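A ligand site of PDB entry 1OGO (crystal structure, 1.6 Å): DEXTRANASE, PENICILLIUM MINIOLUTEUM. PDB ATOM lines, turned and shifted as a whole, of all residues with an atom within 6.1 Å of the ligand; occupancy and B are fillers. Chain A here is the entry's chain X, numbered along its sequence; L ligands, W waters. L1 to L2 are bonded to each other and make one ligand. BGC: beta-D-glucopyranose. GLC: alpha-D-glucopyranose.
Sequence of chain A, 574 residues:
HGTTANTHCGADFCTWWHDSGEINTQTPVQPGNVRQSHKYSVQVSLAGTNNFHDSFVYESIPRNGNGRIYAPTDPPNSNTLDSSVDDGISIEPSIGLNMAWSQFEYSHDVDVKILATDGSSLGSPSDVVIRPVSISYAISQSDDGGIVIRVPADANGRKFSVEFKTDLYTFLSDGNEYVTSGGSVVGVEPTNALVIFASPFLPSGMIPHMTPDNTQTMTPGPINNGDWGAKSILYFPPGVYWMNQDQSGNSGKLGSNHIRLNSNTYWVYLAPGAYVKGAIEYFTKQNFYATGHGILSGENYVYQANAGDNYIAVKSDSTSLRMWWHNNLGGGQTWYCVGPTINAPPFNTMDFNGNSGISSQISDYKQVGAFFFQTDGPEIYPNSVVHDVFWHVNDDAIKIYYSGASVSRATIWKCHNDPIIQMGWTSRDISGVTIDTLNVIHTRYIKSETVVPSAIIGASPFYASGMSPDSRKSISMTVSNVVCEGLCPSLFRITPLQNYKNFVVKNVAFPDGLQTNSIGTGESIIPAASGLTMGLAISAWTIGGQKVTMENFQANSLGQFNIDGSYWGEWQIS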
ATOM      1  N   ASP A  86      21.451  -4.689  -8.616  1.00  0.00           N
ATOM      2  CA  ASP A  86      20.012  -4.861  -8.491  1.00  0.00           C
ATOM      3  C   ASP A  86      19.835  -6.232  -7.872  1.00  0.00           C
ATOM      4  O   ASP A  86      20.175  -7.245  -8.483  1.00  0.00           O
ATOM      5  CB  ASP A  86      19.356  -4.756  -9.875  1.00  0.00           C
ATOM      6  CG  ASP A  86      17.822  -4.795  -9.827  1.00  0.00           C
ATOM      7  OD1 ASP A  86      17.230  -5.041  -8.749  1.00  0.00           O
ATOM      8  OD2 ASP A  86      17.136  -4.605 -10.859  1.00  0.00           O
ATOM      9  N   TYR A 303      22.399 -11.584  -0.194  1.00  0.00           N
ATOM     10  CA  TYR A 303      22.101 -11.895  -1.585  1.00  0.00           C
ATOM     11  C   TYR A 303      23.290 -12.596  -2.248  1.00  0.00           C
ATOM     12  O   TYR A 303      24.427 -12.135  -2.122  1.00  0.00           O
ATOM     13  CB  TYR A 303      21.758 -10.606  -2.297  1.00  0.00           C
ATOM     14  CG  TYR A 303      21.462 -10.752  -3.771  1.00  0.00           C
ATOM     15  CD1 TYR A 303      20.575 -11.724  -4.231  1.00  0.00           C
ATOM     16  CD2 TYR A 303      22.083  -9.931  -4.703  1.00  0.00           C
ATOM     17  CE1 TYR A 303      20.295 -11.858  -5.586  1.00  0.00           C
ATOM     18  CE2 TYR A 303      21.803 -10.066  -6.058  1.00  0.00           C
ATOM     19  CZ  TYR A 303      20.922 -11.033  -6.490  1.00  0.00           C
ATOM     20  OH  TYR A 303      20.622 -11.176  -7.845  1.00  0.00           O
ATOM     21  N   GLN A 304      23.039 -13.733  -2.883  1.00  0.00           N
ATOM     22  CA  GLN A 304      24.055 -14.515  -3.619  1.00  0.00           C
ATOM     23  C   GLN A 304      25.166 -15.102  -2.736  1.00  0.00           C
ATOM     24  O   GLN A 304      26.240 -15.479  -3.259  1.00  0.00           O
ATOM     25  CB  GLN A 304      24.706 -13.661  -4.714  1.00  0.00           C
ATOM     26  CG  GLN A 304      23.757 -13.003  -5.675  1.00  0.00           C
ATOM     27  CD  GLN A 304      24.434 -12.011  -6.641  1.00  0.00           C
ATOM     28  OE1 GLN A 304      25.304 -11.206  -6.247  1.00  0.00           O
ATOM     29  NE2 GLN A 304      24.016 -12.049  -7.883  1.00  0.00           N
ATOM     30  N   LYS A 315      28.326 -13.222  -6.818  1.00  0.00           N
ATOM     31  CA  LYS A 315      27.686 -14.300  -7.531  1.00  0.00           C
ATOM     32  C   LYS A 315      28.710 -15.296  -8.027  1.00  0.00           C
ATOM     33  O   LYS A 315      29.686 -14.897  -8.650  1.00  0.00           O
ATOM     34  CB  LYS A 315      26.932 -13.759  -8.747  1.00  0.00           C
ATOM     35  CG  LYS A 315      26.223 -14.830  -9.530  1.00  0.00           C
ATOM     36  CD  LYS A 315      25.406 -14.244 -10.690  1.00  0.00           C
ATOM     37  CE  LYS A 315      24.922 -15.362 -11.597  1.00  0.00           C
ATOM     38  NZ  LYS A 315      24.046 -14.860 -12.715  1.00  0.00           N
ATOM     39  N   PHE A 373      16.241 -11.678  -6.621  1.00  0.00           N
ATOM     40  CA  PHE A 373      16.499 -12.312  -7.917  1.00  0.00           C
ATOM     41  C   PHE A 373      17.164 -13.673  -7.706  1.00  0.00           C
ATOM     42  O   PHE A 373      17.771 -13.944  -6.663  1.00  0.00           O
ATOM     43  CB  PHE A 373      17.468 -11.488  -8.768  1.00  0.00           C
ATOM     44  CG  PHE A 373      16.881 -10.330  -9.525  1.00  0.00           C
ATOM     45  CD1 PHE A 373      17.712  -9.250  -9.828  1.00  0.00           C
ATOM     46  CD2 PHE A 373      15.581 -10.328 -10.017  1.00  0.00           C
ATOM     47  CE1 PHE A 373      17.247  -8.179 -10.580  1.00  0.00           C
ATOM     48  CE2 PHE A 373      15.116  -9.244 -10.774  1.00  0.00           C
ATOM     49  CZ  PHE A 373      15.952  -8.179 -11.059  1.00  0.00           C
ATOM     50  N   GLN A 374      17.040 -14.527  -8.719  1.00  0.00           N
ATOM     51  CA  GLN A 374      17.766 -15.793  -8.781  1.00  0.00           C
ATOM     52  C   GLN A 374      17.242 -16.877  -7.824  1.00  0.00           C
ATOM     53  O   GLN A 374      17.858 -17.923  -7.664  1.00  0.00           O
ATOM     54  CB  GLN A 374      19.279 -15.558  -8.631  1.00  0.00           C
ATOM     55  CG  GLN A 374      19.817 -14.608  -9.710  1.00  0.00           C
ATOM     56  CD  GLN A 374      21.307 -14.393  -9.663  1.00  0.00           C
ATOM     57  OE1 GLN A 374      21.808 -13.509  -8.948  1.00  0.00           O
ATOM     58  NE2 GLN A 374      22.023 -15.207 -10.404  1.00  0.00           N
ATOM     59  N   ASN A 394      11.380 -15.313  -7.517  1.00  0.00           N
ATOM     60  CA  ASN A 394      11.773 -14.166  -8.316  1.00  0.00           C
ATOM     61  C   ASN A 394      12.818 -14.591  -9.338  1.00  0.00           C
ATOM     62  O   ASN A 394      13.756 -13.857  -9.689  1.00  0.00           O
ATOM     63  CB  ASN A 394      12.228 -12.963  -7.460  1.00  0.00           C
ATOM     64  CG  ASN A 394      12.230 -11.637  -8.231  1.00  0.00           C
ATOM     65  OD1 ASN A 394      11.678 -11.546  -9.342  1.00  0.00           O
ATOM     66  ND2 ASN A 394      12.875 -10.610  -7.660  1.00  0.00           N
ATOM     67  N   ASP A 395      12.632 -15.832  -9.785  1.00  0.00           N
ATOM     68  CA  ASP A 395      13.301 -16.356 -10.970  1.00  0.00           C
ATOM     69  C   ASP A 395      12.566 -17.582 -11.497  1.00  0.00           C
ATOM     70  O   ASP A 395      11.441 -17.871 -11.080  1.00  0.00           O
ATOM     71  CB  ASP A 395      14.779 -16.676 -10.697  1.00  0.00           C
ATOM     72  CG  ASP A 395      15.662 -16.204 -11.819  1.00  0.00           C
ATOM     73  OD1 ASP A 395      15.533 -16.778 -12.930  1.00  0.00           O
ATOM     74  OD2 ASP A 395      16.499 -15.266 -11.692  1.00  0.00           O
ATOM     75  N   ASP A 396      13.190 -18.285 -12.445  1.00  0.00           N
ATOM     76  CA  ASP A 396      12.575 -19.452 -13.098  1.00  0.00           C
ATOM     77  C   ASP A 396      11.866 -20.345 -12.094  1.00  0.00           C
ATOM     78  O   ASP A 396      12.490 -20.796 -11.135  1.00  0.00           O
ATOM     79  CB  ASP A 396      13.645 -20.333 -13.780  1.00  0.00           C
ATOM     80  CG  ASP A 396      14.356 -19.662 -14.930  1.00  0.00           C
ATOM     81  OD1 ASP A 396      13.745 -18.875 -15.692  1.00  0.00           O
ATOM     82  OD2 ASP A 396      15.561 -19.916 -15.184  1.00  0.00           O
ATOM     83  N   ASN A 417      10.811 -11.567 -12.393  1.00  0.00           N
ATOM     84  CA  ASN A 417      11.950 -11.978 -13.204  1.00  0.00           C
ATOM     85  C   ASN A 417      11.844 -13.400 -13.722  1.00  0.00           C
ATOM     86  O   ASN A 417      11.610 -14.327 -12.975  1.00  0.00           O
ATOM     87  CB  ASN A 417      13.217 -11.828 -12.363  1.00  0.00           C
ATOM     88  CG  ASN A 417      14.512 -11.930 -13.194  1.00  0.00           C
ATOM     89  OD1 ASN A 417      14.699 -11.216 -14.174  1.00  0.00           O
ATOM     90  ND2 ASN A 417      15.420 -12.798 -12.770  1.00  0.00           N
ATOM     91  N   ASP A 418      12.045 -13.533 -15.028  1.00  0.00           N
ATOM     92  CA  ASP A 418      12.098 -14.835 -15.708  1.00  0.00           C
ATOM     93  C   ASP A 418      10.711 -15.484 -15.754  1.00  0.00           C
ATOM     94  O   ASP A 418       9.771 -14.977 -15.149  1.00  0.00           O
ATOM     95  CB  ASP A 418      13.177 -15.745 -15.082  1.00  0.00           C
ATOM     96  CG  ASP A 418      14.454 -15.825 -15.933  1.00  0.00           C
ATOM     97  OD1 ASP A 418      14.358 -15.610 -17.158  1.00  0.00           O
ATOM     98  OD2 ASP A 418      15.588 -16.047 -15.463  1.00  0.00           O
ATOM     99  N   TRP A 425      18.152 -21.182 -22.295  1.00  0.00           N
ATOM    100  CA  TRP A 425      19.546 -20.962 -21.843  1.00  0.00           C
ATOM    101  C   TRP A 425      20.538 -21.771 -22.698  1.00  0.00           C
ATOM    102  O   TRP A 425      21.669 -21.341 -22.923  1.00  0.00           O
ATOM    103  CB  TRP A 425      19.751 -21.213 -20.344  1.00  0.00           C
ATOM    104  CG  TRP A 425      18.938 -20.306 -19.393  1.00  0.00           C
ATOM    105  CD1 TRP A 425      18.029 -20.723 -18.467  1.00  0.00           C
ATOM    106  CD2 TRP A 425      19.000 -18.879 -19.281  1.00  0.00           C
ATOM    107  NE1 TRP A 425      17.504 -19.636 -17.798  1.00  0.00           N
ATOM    108  CE2 TRP A 425      18.089 -18.496 -18.275  1.00  0.00           C
ATOM    109  CE3 TRP A 425      19.721 -17.872 -19.937  1.00  0.00           C
ATOM    110  CZ2 TRP A 425      17.878 -17.153 -17.910  1.00  0.00           C
ATOM    111  CZ3 TRP A 425      19.507 -16.520 -19.569  1.00  0.00           C
ATOM    112  CH2 TRP A 425      18.598 -16.192 -18.566  1.00  0.00           C
ATOM    113  N   LYS A 447       9.229  -4.961 -16.368  1.00  0.00           N
ATOM    114  CA  LYS A 447       9.662  -4.838 -17.749  1.00  0.00           C
ATOM    115  C   LYS A 447       9.130  -5.954 -18.652  1.00  0.00           C
ATOM    116  O   LYS A 447       8.919  -7.086 -18.211  1.00  0.00           O
ATOM    117  CB  LYS A 447      11.185  -4.912 -17.810  1.00  0.00           C
ATOM    118  CG  LYS A 447      11.946  -3.881 -16.978  1.00  0.00           C
ATOM    119  CD  LYS A 447      13.445  -4.147 -17.038  1.00  0.00           C
ATOM    120  CE  LYS A 447      14.249  -3.277 -16.079  1.00  0.00           C
ATOM    121  NZ  LYS A 447      15.480  -3.968 -15.581  1.00  0.00           N
ATOM    122  N   GLU A 449      10.313  -8.394 -21.258  1.00  0.00           N
ATOM    123  CA  GLU A 449      11.640  -8.920 -21.600  1.00  0.00           C
ATOM    124  C   GLU A 449      11.579 -10.272 -22.304  1.00  0.00           C
ATOM    125  O   GLU A 449      10.640 -11.042 -22.114  1.00  0.00           O
ATOM    126  CB  GLU A 449      12.496  -9.032 -20.355  1.00  0.00           C
ATOM    127  CG  GLU A 449      12.678  -7.705 -19.628  1.00  0.00           C
ATOM    128  CD  GLU A 449      13.624  -7.787 -18.462  1.00  0.00           C
ATOM    129  OE1 GLU A 449      14.846  -7.585 -18.670  1.00  0.00           O
ATOM    130  OE2 GLU A 449      13.144  -8.026 -17.335  1.00  0.00           O
ATOM    131  N   VAL A 451      15.141 -11.780 -22.975  1.00  0.00           N
ATOM    132  CA  VAL A 451      16.377 -12.366 -22.445  1.00  0.00           C
ATOM    133  C   VAL A 451      16.090 -13.117 -21.143  1.00  0.00           C
ATOM    134  O   VAL A 451      16.591 -14.228 -20.932  1.00  0.00           O
ATOM    135  CB  VAL A 451      17.505 -11.314 -22.264  1.00  0.00           C
ATOM    136  CG1 VAL A 451      18.779 -11.982 -21.748  1.00  0.00           C
ATOM    137  CG2 VAL A 451      17.786 -10.607 -23.578  1.00  0.00           C
ATOM    138  N   VAL A 452      15.265 -12.521 -20.293  1.00  0.00           N
ATOM    139  CA  VAL A 452      14.633 -13.204 -19.178  1.00  0.00           C
ATOM    140  C   VAL A 452      13.134 -13.131 -19.452  1.00  0.00           C
ATOM    141  O   VAL A 452      12.496 -12.111 -19.157  1.00  0.00           O
ATOM    142  CB  VAL A 452      15.010 -12.561 -17.802  1.00  0.00           C
ATOM    143  CG1 VAL A 452      16.359 -13.075 -17.346  1.00  0.00           C
ATOM    144  CG2 VAL A 452      15.013 -11.038 -17.843  1.00  0.00           C
ATOM    145  N   TYR A 463      22.849 -18.538 -22.626  1.00  0.00           N
ATOM    146  CA  TYR A 463      23.473 -17.944 -21.438  1.00  0.00           C
ATOM    147  C   TYR A 463      24.912 -17.557 -21.729  1.00  0.00           C
ATOM    148  O   TYR A 463      25.336 -16.440 -21.462  1.00  0.00           O
ATOM    149  CB  TYR A 463      23.427 -18.914 -20.234  1.00  0.00           C
ATOM    150  CG  TYR A 463      23.943 -18.363 -18.885  1.00  0.00           C
ATOM    151  CD1 TYR A 463      23.509 -17.119 -18.397  1.00  0.00           C
ATOM    152  CD2 TYR A 463      24.840 -19.095 -18.100  1.00  0.00           C
ATOM    153  CE1 TYR A 463      23.978 -16.620 -17.153  1.00  0.00           C
ATOM    154  CE2 TYR A 463      25.312 -18.605 -16.859  1.00  0.00           C
ATOM    155  CZ  TYR A 463      24.871 -17.366 -16.400  1.00  0.00           C
ATOM    156  OH  TYR A 463      25.333 -16.885 -15.179  1.00  0.00           O
HETATM  157  C2  BGC L   1      18.440  -7.357 -17.934  1.00  0.00           C
HETATM  158  C3  BGC L   1      17.598  -6.773 -16.800  1.00  0.00           C
HETATM  159  C4  BGC L   1      17.134  -7.906 -15.891  1.00  0.00           C
HETATM  160  C5  BGC L   1      18.334  -8.757 -15.461  1.00  0.00           C
HETATM  161  C6  BGC L   1      17.970  -9.934 -14.569  1.00  0.00           C
HETATM  162  C1  BGC L   1      19.555  -8.266 -17.401  1.00  0.00           C
HETATM  163  O1  BGC L   1      20.234  -8.894 -18.467  1.00  0.00           O
HETATM  164  O2  BGC L   1      18.990  -6.315 -18.700  1.00  0.00           O
HETATM  165  O3  BGC L   1      16.516  -6.028 -17.343  1.00  0.00           O
HETATM  166  O4  BGC L   1      16.485  -7.369 -14.751  1.00  0.00           O
HETATM  167  O5  BGC L   1      19.014  -9.277 -16.579  1.00  0.00           O
HETATM  168  O6  BGC L   1      19.183 -10.338 -13.969  1.00  0.00           O
HETATM  169  C1  GLC L   2      18.990 -11.260 -12.882  1.00  0.00           C
HETATM  170  C2  GLC L   2      20.326 -11.427 -12.162  1.00  0.00           C
HETATM  171  C3  GLC L   2      21.281 -12.288 -13.009  1.00  0.00           C
HETATM  172  C4  GLC L   2      20.611 -13.596 -13.446  1.00  0.00           C
HETATM  173  C5  GLC L   2      19.281 -13.279 -14.136  1.00  0.00           C
HETATM  174  C6  GLC L   2      18.545 -14.555 -14.548  1.00  0.00           C
HETATM  175  O2  GLC L   2      20.877 -10.141 -11.973  1.00  0.00           O
HETATM  176  O3  GLC L   2      22.451 -12.593 -12.282  1.00  0.00           O
HETATM  177  O4  GLC L   2      21.476 -14.303 -14.324  1.00  0.00           O
HETATM  178  O5  GLC L   2      18.466 -12.514 -13.269  1.00  0.00           O
HETATM  179  O6  GLC L   2      18.426 -15.447 -13.463  1.00  0.00           O
HETATM  180  O   HOH W   1      21.658  -9.192  -9.429  1.00  0.00           O
HETATM  181  O   HOH W   2      20.553  -7.487 -12.373  1.00  0.00           O
HETATM  182  O   HOH W   3      18.489 -18.150 -11.625  1.00  0.00           O
HETATM  183  O   HOH W   4      14.202  -8.587 -14.916  1.00  0.00           O
HETATM  184  O   HOH W   5      18.178  -5.740 -13.105  1.00  0.00           O
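OD2 of Asp 395 sits at hydrogen-bond distance from ND2 of Asn 417, 2.9 Å away.
OD2 of Asp 395 sits at hydrogen-bond distance from N of Gln 374, at 3.1 Å.
The side-chain carboxylate (OD1) of Asp 395 sits close to the side-chain carboxylate (OD2) of Asp 418 (2.6 Å).
OH of Tyr 463 is in hydrogen-bond range of NZ of Lys 315.
OD1 of Asn 394 is in hydrogen-bond range of N of Asn 417 (3.2 Å).
OH of Tyr 303 sits at hydrogen-bond distance from OE1 of Gln 374 (2.8 Å).
OE1 of Gln 374 is in hydrogen-bond range of NE2 of Gln 304, 2.9 Å away.
N of Gln 374 lies within hydrogen-bond range of O of Asn 394 (3.5 Å).
Merely in contact with the ligand: Phe 373 (3.8 Å), Asp 418 (3.4 Å) and Val 452 (3.8 Å).
Hydrophobic or aromatic side chains that line the ligand: Phe 373 and Val 452.
The nearest printed residue that does not touch the ligand is Tyr 303 (4.3 Å).
Water W4 lies within hydrogen-bond range of an oxygen (O4) of BGC L1 (2.6 Å), the side-chain carboxylate of Glu 449 (2.7 Å) and the side-chain amide oxygen of Asn 417 (2.8 Å).
Water W1 lies within hydrogen-bond range of the backbone carbonyl oxygen (O) of Asp 86, the side-chain hydroxyl (OH) of Tyr 303 and an oxygen (O2) of GLC L2.
Water W5 bridges the side-chain carboxylate of Asp 86 (2.7 Å) and an oxygen (O4) of BGC L1 (2.9 Å).
An oxygen (O6) of GLC L2 is in hydrogen-bond range of the side-chain carboxylate of Asp 395, at 2.6 Å.
An oxygen (O3) of BGC L1 lies within hydrogen-bond range of the side-chain carboxylate (OE1) of Glu 449 (2.6 Å).
An oxygen (O3) of GLC L2 sits at hydrogen-bond distance from the side-chain amino group (NZ) of Lys 315 (2.8 Å).
O3 of BGC L1 is in hydrogen-bond range of NZ of Lys 447.
ND2 of Asn 417 sits at hydrogen-bond distance from O5 of GLC L2 (3.1 Å).
The side-chain amide nitrogen of Gln 374 is in hydrogen-bond range of an oxygen (O3) of GLC L2 (3.2 Å).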
